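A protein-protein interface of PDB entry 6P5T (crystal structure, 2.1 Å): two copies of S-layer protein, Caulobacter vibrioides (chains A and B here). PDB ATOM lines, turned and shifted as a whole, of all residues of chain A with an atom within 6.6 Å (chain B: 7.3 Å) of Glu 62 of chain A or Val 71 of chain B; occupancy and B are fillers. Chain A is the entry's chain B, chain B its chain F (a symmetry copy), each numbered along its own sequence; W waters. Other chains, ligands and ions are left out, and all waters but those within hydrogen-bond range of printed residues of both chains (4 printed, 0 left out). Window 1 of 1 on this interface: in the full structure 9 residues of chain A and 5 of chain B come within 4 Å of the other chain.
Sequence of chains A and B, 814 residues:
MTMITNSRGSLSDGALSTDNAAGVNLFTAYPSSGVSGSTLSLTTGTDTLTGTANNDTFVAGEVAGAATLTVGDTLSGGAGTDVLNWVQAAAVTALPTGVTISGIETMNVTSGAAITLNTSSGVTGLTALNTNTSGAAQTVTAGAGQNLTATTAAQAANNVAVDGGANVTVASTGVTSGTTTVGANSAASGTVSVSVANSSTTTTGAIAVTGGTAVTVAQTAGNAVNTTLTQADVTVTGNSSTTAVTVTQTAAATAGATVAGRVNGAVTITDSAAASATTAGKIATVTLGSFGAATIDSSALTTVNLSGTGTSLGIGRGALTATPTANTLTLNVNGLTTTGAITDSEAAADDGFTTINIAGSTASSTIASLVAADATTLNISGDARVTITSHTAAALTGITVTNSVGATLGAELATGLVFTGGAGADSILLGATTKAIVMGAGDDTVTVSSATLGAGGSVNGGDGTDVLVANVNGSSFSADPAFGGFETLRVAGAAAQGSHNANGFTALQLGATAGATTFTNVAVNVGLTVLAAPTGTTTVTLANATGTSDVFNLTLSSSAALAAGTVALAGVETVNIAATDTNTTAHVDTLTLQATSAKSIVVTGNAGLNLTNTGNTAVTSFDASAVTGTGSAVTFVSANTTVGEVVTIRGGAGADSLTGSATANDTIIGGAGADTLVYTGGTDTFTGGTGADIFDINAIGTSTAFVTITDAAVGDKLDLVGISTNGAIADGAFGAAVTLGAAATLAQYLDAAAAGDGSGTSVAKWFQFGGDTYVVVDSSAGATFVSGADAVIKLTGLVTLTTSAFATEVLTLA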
ATOM      1  N   ALA A  60     -17.414   4.309  20.218  1.00  0.00           N
ATOM      2  CA  ALA A  60     -17.927   2.955  20.223  1.00  0.00           C
ATOM      3  C   ALA A  60     -18.766   2.682  21.457  1.00  0.00           C
ATOM      4  O   ALA A  60     -18.625   1.622  22.075  1.00  0.00           O
ATOM      5  CB  ALA A  60     -16.774   1.947  20.138  1.00  0.00           C
ATOM      6  N   GLY A  61     -19.713   3.563  21.761  1.00  0.00           N
ATOM      7  CA  GLY A  61     -20.613   3.352  22.871  1.00  0.00           C
ATOM      8  C   GLY A  61     -21.791   2.516  22.423  1.00  0.00           C
ATOM      9  O   GLY A  61     -21.755   1.851  21.384  1.00  0.00           O
ATOM     10  N   GLU A  62     -22.894   2.651  23.135  1.00  0.00           N
ATOM     11  CA  GLU A  62     -24.045   1.835  22.800  1.00  0.00           C
ATOM     12  C   GLU A  62     -24.982   2.608  21.894  1.00  0.00           C
ATOM     13  O   GLU A  62     -25.032   3.842  21.918  1.00  0.00           O
ATOM     14  CB  GLU A  62     -24.796   1.391  24.054  1.00  0.00           C
ATOM     15  CG  GLU A  62     -24.110   0.292  24.828  1.00  0.00           C
ATOM     16  CD  GLU A  62     -24.903  -0.138  26.052  1.00  0.00           C
ATOM     17  OE1 GLU A  62     -25.431   0.742  26.779  1.00  0.00           O
ATOM     18  OE2 GLU A  62     -24.985  -1.365  26.293  1.00  0.00           O
ATOM     19  N   VAL A  63     -25.669   1.853  21.042  1.00  0.00           N
ATOM     20  CA  VAL A  63     -26.764   2.341  20.218  1.00  0.00           C
ATOM     21  C   VAL A  63     -27.989   1.518  20.590  1.00  0.00           C
ATOM     22  O   VAL A  63     -28.042   0.313  20.310  1.00  0.00           O
ATOM     23  CB  VAL A  63     -26.466   2.229  18.718  1.00  0.00           C
ATOM     24  CG1 VAL A  63     -27.736   2.515  17.930  1.00  0.00           C
ATOM     25  CG2 VAL A  63     -25.372   3.200  18.329  1.00  0.00           C
ATOM     26  N   ALA A  64     -28.955   2.158  21.253  1.00  0.00           N
ATOM     27  CA  ALA A  64     -30.195   1.501  21.661  1.00  0.00           C
ATOM     28  C   ALA A  64     -29.921   0.251  22.493  1.00  0.00           C
ATOM     29  O   ALA A  64     -30.556  -0.792  22.307  1.00  0.00           O
ATOM     30  CB  ALA A  64     -31.067   1.166  20.450  1.00  0.00           C
ATOM     31  N   GLY A  65     -28.941   0.343  23.392  1.00  0.00           N
ATOM     32  CA  GLY A  65     -28.630  -0.730  24.314  1.00  0.00           C
ATOM     33  C   GLY A  65     -27.700  -1.799  23.784  1.00  0.00           C
ATOM     34  O   GLY A  65     -27.379  -2.738  24.524  1.00  0.00           O
ATOM     35  N   ALA A  66     -27.261  -1.695  22.531  1.00  0.00           N
ATOM     36  CA  ALA A  66     -26.420  -2.694  21.889  1.00  0.00           C
ATOM     37  C   ALA A  66     -25.016  -2.157  21.632  1.00  0.00           C
ATOM     38  O   ALA A  66     -24.848  -1.021  21.172  1.00  0.00           O
ATOM     39  CB  ALA A  66     -27.050  -3.157  20.571  1.00  0.00           C
ATOM     40  N   ALA A  67     -24.015  -2.992  21.914  1.00  0.00           N
ATOM     41  CA  ALA A  67     -22.614  -2.631  21.715  1.00  0.00           C
ATOM     42  C   ALA A  67     -22.307  -2.409  20.234  1.00  0.00           C
ATOM     43  O   ALA A  67     -22.903  -3.029  19.352  1.00  0.00           O
ATOM     44  CB  ALA A  67     -21.710  -3.732  22.263  1.00  0.00           C
ATOM     45  N   THR A  68     -21.393  -1.479  19.962  1.00  0.00           N
ATOM     46  CA  THR A  68     -20.974  -1.177  18.597  1.00  0.00           C
ATOM     47  C   THR A  68     -19.538  -1.582  18.274  1.00  0.00           C
ATOM     48  O   THR A  68     -19.130  -1.441  17.117  1.00  0.00           O
ATOM     49  CB  THR A  68     -21.139   0.318  18.302  1.00  0.00           C
ATOM     50  OG1 THR A  68     -20.358   1.067  19.241  1.00  0.00           O
ATOM     51  CG2 THR A  68     -22.615   0.733  18.390  1.00  0.00           C
ATOM     52  N   VAL A  87     -17.788   1.432  25.151  1.00  0.00           N
ATOM     53  CA  VAL A  87     -18.691   1.371  26.296  1.00  0.00           C
ATOM     54  C   VAL A  87     -19.835   0.415  25.978  1.00  0.00           C
ATOM     55  O   VAL A  87     -20.476   0.544  24.933  1.00  0.00           O
ATOM     56  CB  VAL A  87     -19.273   2.758  26.646  1.00  0.00           C
ATOM     57  CG1 VAL A  87     -20.297   2.629  27.770  1.00  0.00           C
ATOM     58  CG2 VAL A  87     -18.179   3.750  27.030  1.00  0.00           C
ATOM     59  N   GLN A  88     -20.116  -0.517  26.889  1.00  0.00           N
ATOM     60  CA  GLN A  88     -21.238  -1.425  26.715  1.00  0.00           C
ATOM     61  C   GLN A  88     -21.675  -1.920  28.087  1.00  0.00           C
ATOM     62  O   GLN A  88     -20.843  -2.124  28.970  1.00  0.00           O
ATOM     63  CB  GLN A  88     -20.886  -2.613  25.805  1.00  0.00           C
ATOM     64  CG  GLN A  88     -19.886  -3.610  26.403  1.00  0.00           C
ATOM     65  CD  GLN A  88     -19.573  -4.739  25.441  1.00  0.00           C
ATOM     66  OE1 GLN A  88     -19.210  -4.486  24.302  1.00  0.00           O
ATOM     67  NE2 GLN A  88     -19.705  -5.986  25.897  1.00  0.00           N
ATOM     68  N   ALA A  89     -22.991  -2.108  28.253  1.00  0.00           N
ATOM     69  CA  ALA A  89     -23.531  -2.576  29.527  1.00  0.00           C
ATOM     70  C   ALA A  89     -23.181  -4.030  29.776  1.00  0.00           C
ATOM     71  O   ALA A  89     -22.873  -4.419  30.907  1.00  0.00           O
ATOM     72  CB  ALA A  89     -25.056  -2.400  29.554  1.00  0.00           C
ATOM     73  N   ALA A  90     -23.281  -4.859  28.745  1.00  0.00           N
ATOM     74  CA  ALA A  90     -22.971  -6.268  28.881  1.00  0.00           C
ATOM     75  C   ALA A  90     -21.479  -6.445  29.154  1.00  0.00           C
ATOM     76  O   ALA A  90     -20.656  -5.593  28.816  1.00  0.00           O
ATOM     77  CB  ALA A  90     -23.387  -7.022  27.609  1.00  0.00           C
ATOM     78  N   THR A 110     -15.162   0.452  29.034  1.00  0.00           N
ATOM     79  CA  THR A 110     -16.044   0.573  30.193  1.00  0.00           C
ATOM     80  C   THR A 110     -17.202  -0.397  30.048  1.00  0.00           C
ATOM     81  O   THR A 110     -17.910  -0.379  29.034  1.00  0.00           O
ATOM     82  CB  THR A 110     -16.583   1.999  30.342  1.00  0.00           C
ATOM     83  OG1 THR A 110     -15.487   2.905  30.513  1.00  0.00           O
ATOM     84  CG2 THR A 110     -17.519   2.104  31.553  1.00  0.00           C
ATOM     85  N   SER A 111     -17.420  -1.222  31.065  1.00  0.00           N
ATOM     86  CA  SER A 111     -18.516  -2.175  31.020  1.00  0.00           C
ATOM     87  C   SER A 111     -19.388  -2.047  32.260  1.00  0.00           C
ATOM     88  O   SER A 111     -18.938  -1.601  33.323  1.00  0.00           O
ATOM     89  CB  SER A 111     -17.996  -3.616  30.912  1.00  0.00           C
ATOM     90  OG  SER A 111     -19.050  -4.559  30.924  1.00  0.00           O
ATOM     91  N   GLY A 112     -20.654  -2.424  32.099  1.00  0.00           N
ATOM     92  CA  GLY A 112     -21.552  -2.538  33.227  1.00  0.00           C
ATOM     93  C   GLY A 112     -21.388  -3.823  33.998  1.00  0.00           C
ATOM     94  O   GLY A 112     -21.979  -3.976  35.071  1.00  0.00           O
ATOM     95  N   THR B  43     -30.857   8.744  25.468  1.00  0.00           N
ATOM     96  CA  THR B  43     -31.328   7.540  24.796  1.00  0.00           C
ATOM     97  C   THR B  43     -30.896   6.310  25.582  1.00  0.00           C
ATOM     98  O   THR B  43     -30.145   6.396  26.563  1.00  0.00           O
ATOM     99  CB  THR B  43     -30.787   7.442  23.360  1.00  0.00           C
ATOM    100  OG1 THR B  43     -29.412   7.022  23.394  1.00  0.00           O
ATOM    101  CG2 THR B  43     -30.877   8.796  22.661  1.00  0.00           C
ATOM    102  N   THR B  44     -31.370   5.151  25.124  1.00  0.00           N
ATOM    103  CA  THR B  44     -30.949   3.873  25.684  1.00  0.00           C
ATOM    104  C   THR B  44     -29.559   3.458  25.224  1.00  0.00           C
ATOM    105  O   THR B  44     -29.066   2.420  25.672  1.00  0.00           O
ATOM    106  CB  THR B  44     -31.961   2.779  25.340  1.00  0.00           C
ATOM    107  OG1 THR B  44     -31.976   2.557  23.920  1.00  0.00           O
ATOM    108  CG2 THR B  44     -33.361   3.171  25.831  1.00  0.00           C
ATOM    109  N   GLY B  45     -28.943   4.209  24.310  1.00  0.00           N
ATOM    110  CA  GLY B  45     -27.545   4.030  23.970  1.00  0.00           C
ATOM    111  C   GLY B  45     -26.686   4.920  24.861  1.00  0.00           C
ATOM    112  O   GLY B  45     -27.173   5.554  25.795  1.00  0.00           O
ATOM    113  N   THR B  46     -25.381   4.960  24.562  1.00  0.00           N
ATOM    114  CA  THR B  46     -24.447   5.806  25.311  1.00  0.00           C
ATOM    115  C   THR B  46     -24.488   7.229  24.766  1.00  0.00           C
ATOM    116  O   THR B  46     -24.187   7.444  23.593  1.00  0.00           O
ATOM    117  CB  THR B  46     -23.022   5.263  25.224  1.00  0.00           C
ATOM    118  OG1 THR B  46     -23.008   3.882  25.613  1.00  0.00           O
ATOM    119  CG2 THR B  46     -22.076   6.080  26.169  1.00  0.00           C
ATOM    120  N   ASP B  47     -24.878   8.203  25.593  1.00  0.00           N
ATOM    121  CA  ASP B  47     -25.026   9.573  25.115  1.00  0.00           C
ATOM    122  C   ASP B  47     -23.867  10.454  25.558  1.00  0.00           C
ATOM    123  O   ASP B  47     -23.351  10.321  26.667  1.00  0.00           O
ATOM    124  CB  ASP B  47     -26.337  10.187  25.609  1.00  0.00           C
ATOM    125  CG  ASP B  47     -27.524   9.294  25.348  1.00  0.00           C
ATOM    126  OD1 ASP B  47     -28.118   8.790  26.330  1.00  0.00           O
ATOM    127  OD2 ASP B  47     -27.830   9.074  24.143  1.00  0.00           O
ATOM    128  N   THR B  68     -32.870   5.621  30.248  1.00  0.00           N
ATOM    129  CA  THR B  68     -31.974   6.271  29.309  1.00  0.00           C
ATOM    130  C   THR B  68     -30.720   6.839  29.962  1.00  0.00           C
ATOM    131  O   THR B  68     -29.788   7.210  29.245  1.00  0.00           O
ATOM    132  CB  THR B  68     -32.698   7.415  28.584  1.00  0.00           C
ATOM    133  OG1 THR B  68     -33.092   8.408  29.541  1.00  0.00           O
ATOM    134  CG2 THR B  68     -33.943   6.898  27.835  1.00  0.00           C
ATOM    135  N   LEU B  69     -30.669   6.933  31.290  1.00  0.00           N
ATOM    136  CA  LEU B  69     -29.407   7.208  31.972  1.00  0.00           C
ATOM    137  C   LEU B  69     -28.690   5.876  32.118  1.00  0.00           C
ATOM    138  O   LEU B  69     -29.131   5.004  32.874  1.00  0.00           O
ATOM    139  CB  LEU B  69     -29.630   7.881  33.329  1.00  0.00           C
ATOM    140  CG  LEU B  69     -28.348   8.404  33.986  1.00  0.00           C
ATOM    141  CD1 LEU B  69     -27.682   9.448  33.114  1.00  0.00           C
ATOM    142  CD2 LEU B  69     -28.636   8.993  35.340  1.00  0.00           C
ATOM    143  N   THR B  70     -27.625   5.686  31.343  1.00  0.00           N
ATOM    144  CA  THR B  70     -27.055   4.365  31.146  1.00  0.00           C
ATOM    145  C   THR B  70     -25.540   4.472  31.263  1.00  0.00           C
ATOM    146  O   THR B  70     -24.979   5.570  31.325  1.00  0.00           O
ATOM    147  CB  THR B  70     -27.445   3.775  29.776  1.00  0.00           C
ATOM    148  OG1 THR B  70     -27.213   4.744  28.736  1.00  0.00           O
ATOM    149  CG2 THR B  70     -28.937   3.404  29.757  1.00  0.00           C
ATOM    150  N   VAL B  71     -24.887   3.306  31.278  1.00  0.00           N
ATOM    151  CA  VAL B  71     -23.451   3.226  31.499  1.00  0.00           C
ATOM    152  C   VAL B  71     -22.731   4.142  30.519  1.00  0.00           C
ATOM    153  O   VAL B  71     -23.012   4.132  29.316  1.00  0.00           O
ATOM    154  CB  VAL B  71     -22.985   1.763  31.367  1.00  0.00           C
ATOM    155  CG1 VAL B  71     -23.382   1.182  29.996  1.00  0.00           C
ATOM    156  CG2 VAL B  71     -21.485   1.642  31.583  1.00  0.00           C
ATOM    157  N   GLY B  72     -21.827   4.975  31.041  1.00  0.00           N
ATOM    158  CA  GLY B  72     -20.968   5.775  30.191  1.00  0.00           C
ATOM    159  C   GLY B  72     -21.543   7.091  29.720  1.00  0.00           C
ATOM    160  O   GLY B  72     -20.846   7.818  28.999  1.00  0.00           O
ATOM    161  N   ASP B  73     -22.808   7.392  30.037  1.00  0.00           N
ATOM    162  CA  ASP B  73     -23.416   8.647  29.601  1.00  0.00           C
ATOM    163  C   ASP B  73     -22.578   9.823  30.095  1.00  0.00           C
ATOM    164  O   ASP B  73     -22.054   9.794  31.210  1.00  0.00           O
ATOM    165  CB  ASP B  73     -24.848   8.773  30.142  1.00  0.00           C
ATOM    166  CG  ASP B  73     -25.901   8.017  29.303  1.00  0.00           C
ATOM    167  OD1 ASP B  73     -27.055   7.897  29.787  1.00  0.00           O
ATOM    168  OD2 ASP B  73     -25.609   7.529  28.176  1.00  0.00           O
ATOM    169  N   THR B  74     -22.437  10.856  29.259  1.00  0.00           N
ATOM    170  CA  THR B  74     -21.683  12.059  29.609  1.00  0.00           C
ATOM    171  C   THR B  74     -22.531  13.301  29.360  1.00  0.00           C
ATOM    172  O   THR B  74     -22.967  13.543  28.228  1.00  0.00           O
ATOM    173  CB  THR B  74     -20.376  12.138  28.813  1.00  0.00           C
ATOM    174  OG1 THR B  74     -19.539  11.036  29.186  1.00  0.00           O
ATOM    175  CG2 THR B  74     -19.651  13.433  29.098  1.00  0.00           C
ATOM    176  N   PRO B  96     -25.344   5.258  37.153  1.00  0.00           N
ATOM    177  CA  PRO B  96     -24.805   4.074  36.474  1.00  0.00           C
ATOM    178  C   PRO B  96     -23.300   4.200  36.269  1.00  0.00           C
ATOM    179  O   PRO B  96     -22.743   5.297  36.201  1.00  0.00           O
ATOM    180  CB  PRO B  96     -25.543   4.065  35.132  1.00  0.00           C
ATOM    181  CG  PRO B  96     -26.821   4.781  35.400  1.00  0.00           C
ATOM    182  CD  PRO B  96     -26.491   5.841  36.435  1.00  0.00           C
ATOM    183  N   THR B  97     -22.648   3.047  36.129  1.00  0.00           N
ATOM    184  CA  THR B  97     -21.200   2.994  35.935  1.00  0.00           C
ATOM    185  C   THR B  97     -20.747   3.921  34.811  1.00  0.00           C
ATOM    186  O   THR B  97     -21.349   3.961  33.734  1.00  0.00           O
ATOM    187  CB  THR B  97     -20.770   1.555  35.638  1.00  0.00           C
ATOM    188  OG1 THR B  97     -21.098   0.713  36.748  1.00  0.00           O
ATOM    189  CG2 THR B  97     -19.265   1.465  35.363  1.00  0.00           C
ATOM    190  N   GLY B  98     -19.698   4.698  35.087  1.00  0.00           N
ATOM    191  CA  GLY B  98     -19.045   5.523  34.088  1.00  0.00           C
ATOM    192  C   GLY B  98     -19.781   6.787  33.714  1.00  0.00           C
ATOM    193  O   GLY B  98     -19.342   7.491  32.793  1.00  0.00           O
ATOM    194  N   VAL B  99     -20.848   7.131  34.429  1.00  0.00           N
ATOM    195  CA  VAL B  99     -21.629   8.321  34.115  1.00  0.00           C
ATOM    196  C   VAL B  99     -20.897   9.554  34.618  1.00  0.00           C
ATOM    197  O   VAL B  99     -20.383   9.570  35.739  1.00  0.00           O
ATOM    198  CB  VAL B  99     -23.039   8.220  34.727  1.00  0.00           C
ATOM    199  CG1 VAL B  99     -23.652   9.608  34.888  1.00  0.00           C
ATOM    200  CG2 VAL B  99     -23.925   7.336  33.844  1.00  0.00           C
HETATM  201  O   HOH W   1     -29.287   5.270  20.813  1.00  0.00           O
HETATM  202  O   HOH W   2     -21.333  -2.023  36.937  1.00  0.00           O
HETATM  203  O   HOH W   3     -23.577   5.993  20.755  1.00  0.00           O
HETATM  204  O   HOH W   4     -24.941   3.545  27.677  1.00  0.00           O
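Of the 16 printed residues of chain A, 8 touch a printed residue of chain B. Hydrophobic or aromatic side chains of chain A within 4 Å of the printed part of chain B: Ala 64, Val 87 and Ala 89. Among the printed residues, no Asp or Glu carboxylate lies within 4 Å of a Lys or Arg side-chain nitrogen of the other chain.
Water W4 lies within hydrogen-bond range of the backbone carbonyl oxygen of Val 71 of chain B, the side-chain hydroxyl of Thr 46 of chain B and the side-chain carboxylate of Glu 62 of chain A. Water W2 lies within hydrogen-bond range of the side-chain hydroxyl of Thr 97 of chain B and the backbone carbonyl oxygen of Gly 112 of chain A. Water W3 lies within hydrogen-bond range of O of Glu 62 of chain A and O of Thr 46 of chain B. Water W1 lies within hydrogen-bond range of OG1 of Thr 43 of chain B and N of Ala 64 of chain A.
Of the printed residues of chain B, Gly 61 of chain A touches Thr 46. Glu 62 of chain A touches just these residues of chain B: Gly 45 (3.2 Å), Thr 46 (2.8 Å) and Val 71 (3.8 Å). Val 63 of chain A touches none of the printed residues of chain B. Of the printed residues of chain B, Ala 89 of chain A touches Val 71. Of the printed residues of chain A, Thr 46 of chain B touches Gly 61, Glu 62 and Val 87. Printed residues of chain A within 4 Å of Val 71 of chain B: Glu 62 (3.8 Å), Val 87 (3.5 Å), Ala 89 (3.7 Å) and Thr 110 (3.99 Å). The nearest printed residue of chain A that does not touch Thr 46 of chain B is Val 63 of chain A (4.7 Å).
The backbone NH (N) of Val 87 of chain A lies within hydrogen-bond range of the backbone carbonyl oxygen (O) of Ala 60 of chain A (3.2 Å). The backbone carbonyl oxygen of Gly 61 of chain A lies within hydrogen-bond range of the side-chain hydroxyl of Thr 68 of chain A. N of Ala 89 of chain A lies within hydrogen-bond range of OE2 of Glu 62 of chain A, 2.9 Å away. The backbone carbonyl oxygen (O) of Ala 89 of chain A is in hydrogen-bond range of the backbone NH (N) of Gly 112 of chain A, at 3.2 Å. OG of Ser 111 of chain A sits at hydrogen-bond distance from O of Ala 90 of chain A (2.8 Å). The backbone NH of Gly 72 of chain B sits at hydrogen-bond distance from the backbone carbonyl oxygen of Thr 97 of chain B (2.9 Å).
Position printed for both chains: 68. Of the 13 pairs that touch across the chains among the printed residues, none has its exchanged pair printed and touching as well.
The side-chain hydroxyl of Thr 46 of chain B lies within hydrogen-bond range of the backbone NH of Glu 62 of chain A, at 2.8 Å. O of Thr 44 of chain B is in hydrogen-bond range of N of Gly 65 of chain A, at 3.1 Å.
Among the printed residues, merely in contact across the chains: Ala 64 of chain A with Thr 44 of chain B, Glu 62 of chain A with Gly 45 of chain B, Val 87 of chain A with Val 71 of chain B, Ala 64 of chain A with Gly 45 of chain B, Gly 61 of chain A with Thr 46 of chain B, Val 87 of chain A with Thr 46 of chain B, Ser 111 of chain A with Thr 97 of chain B, Ala 89 of chain A with Val 71 of chain B, Glu 62 of chain A with Val 71 of chain B, Gly 65 of chain A with Gly 45 of chain B and Thr 110 of chain A with Val 71 of chain B.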
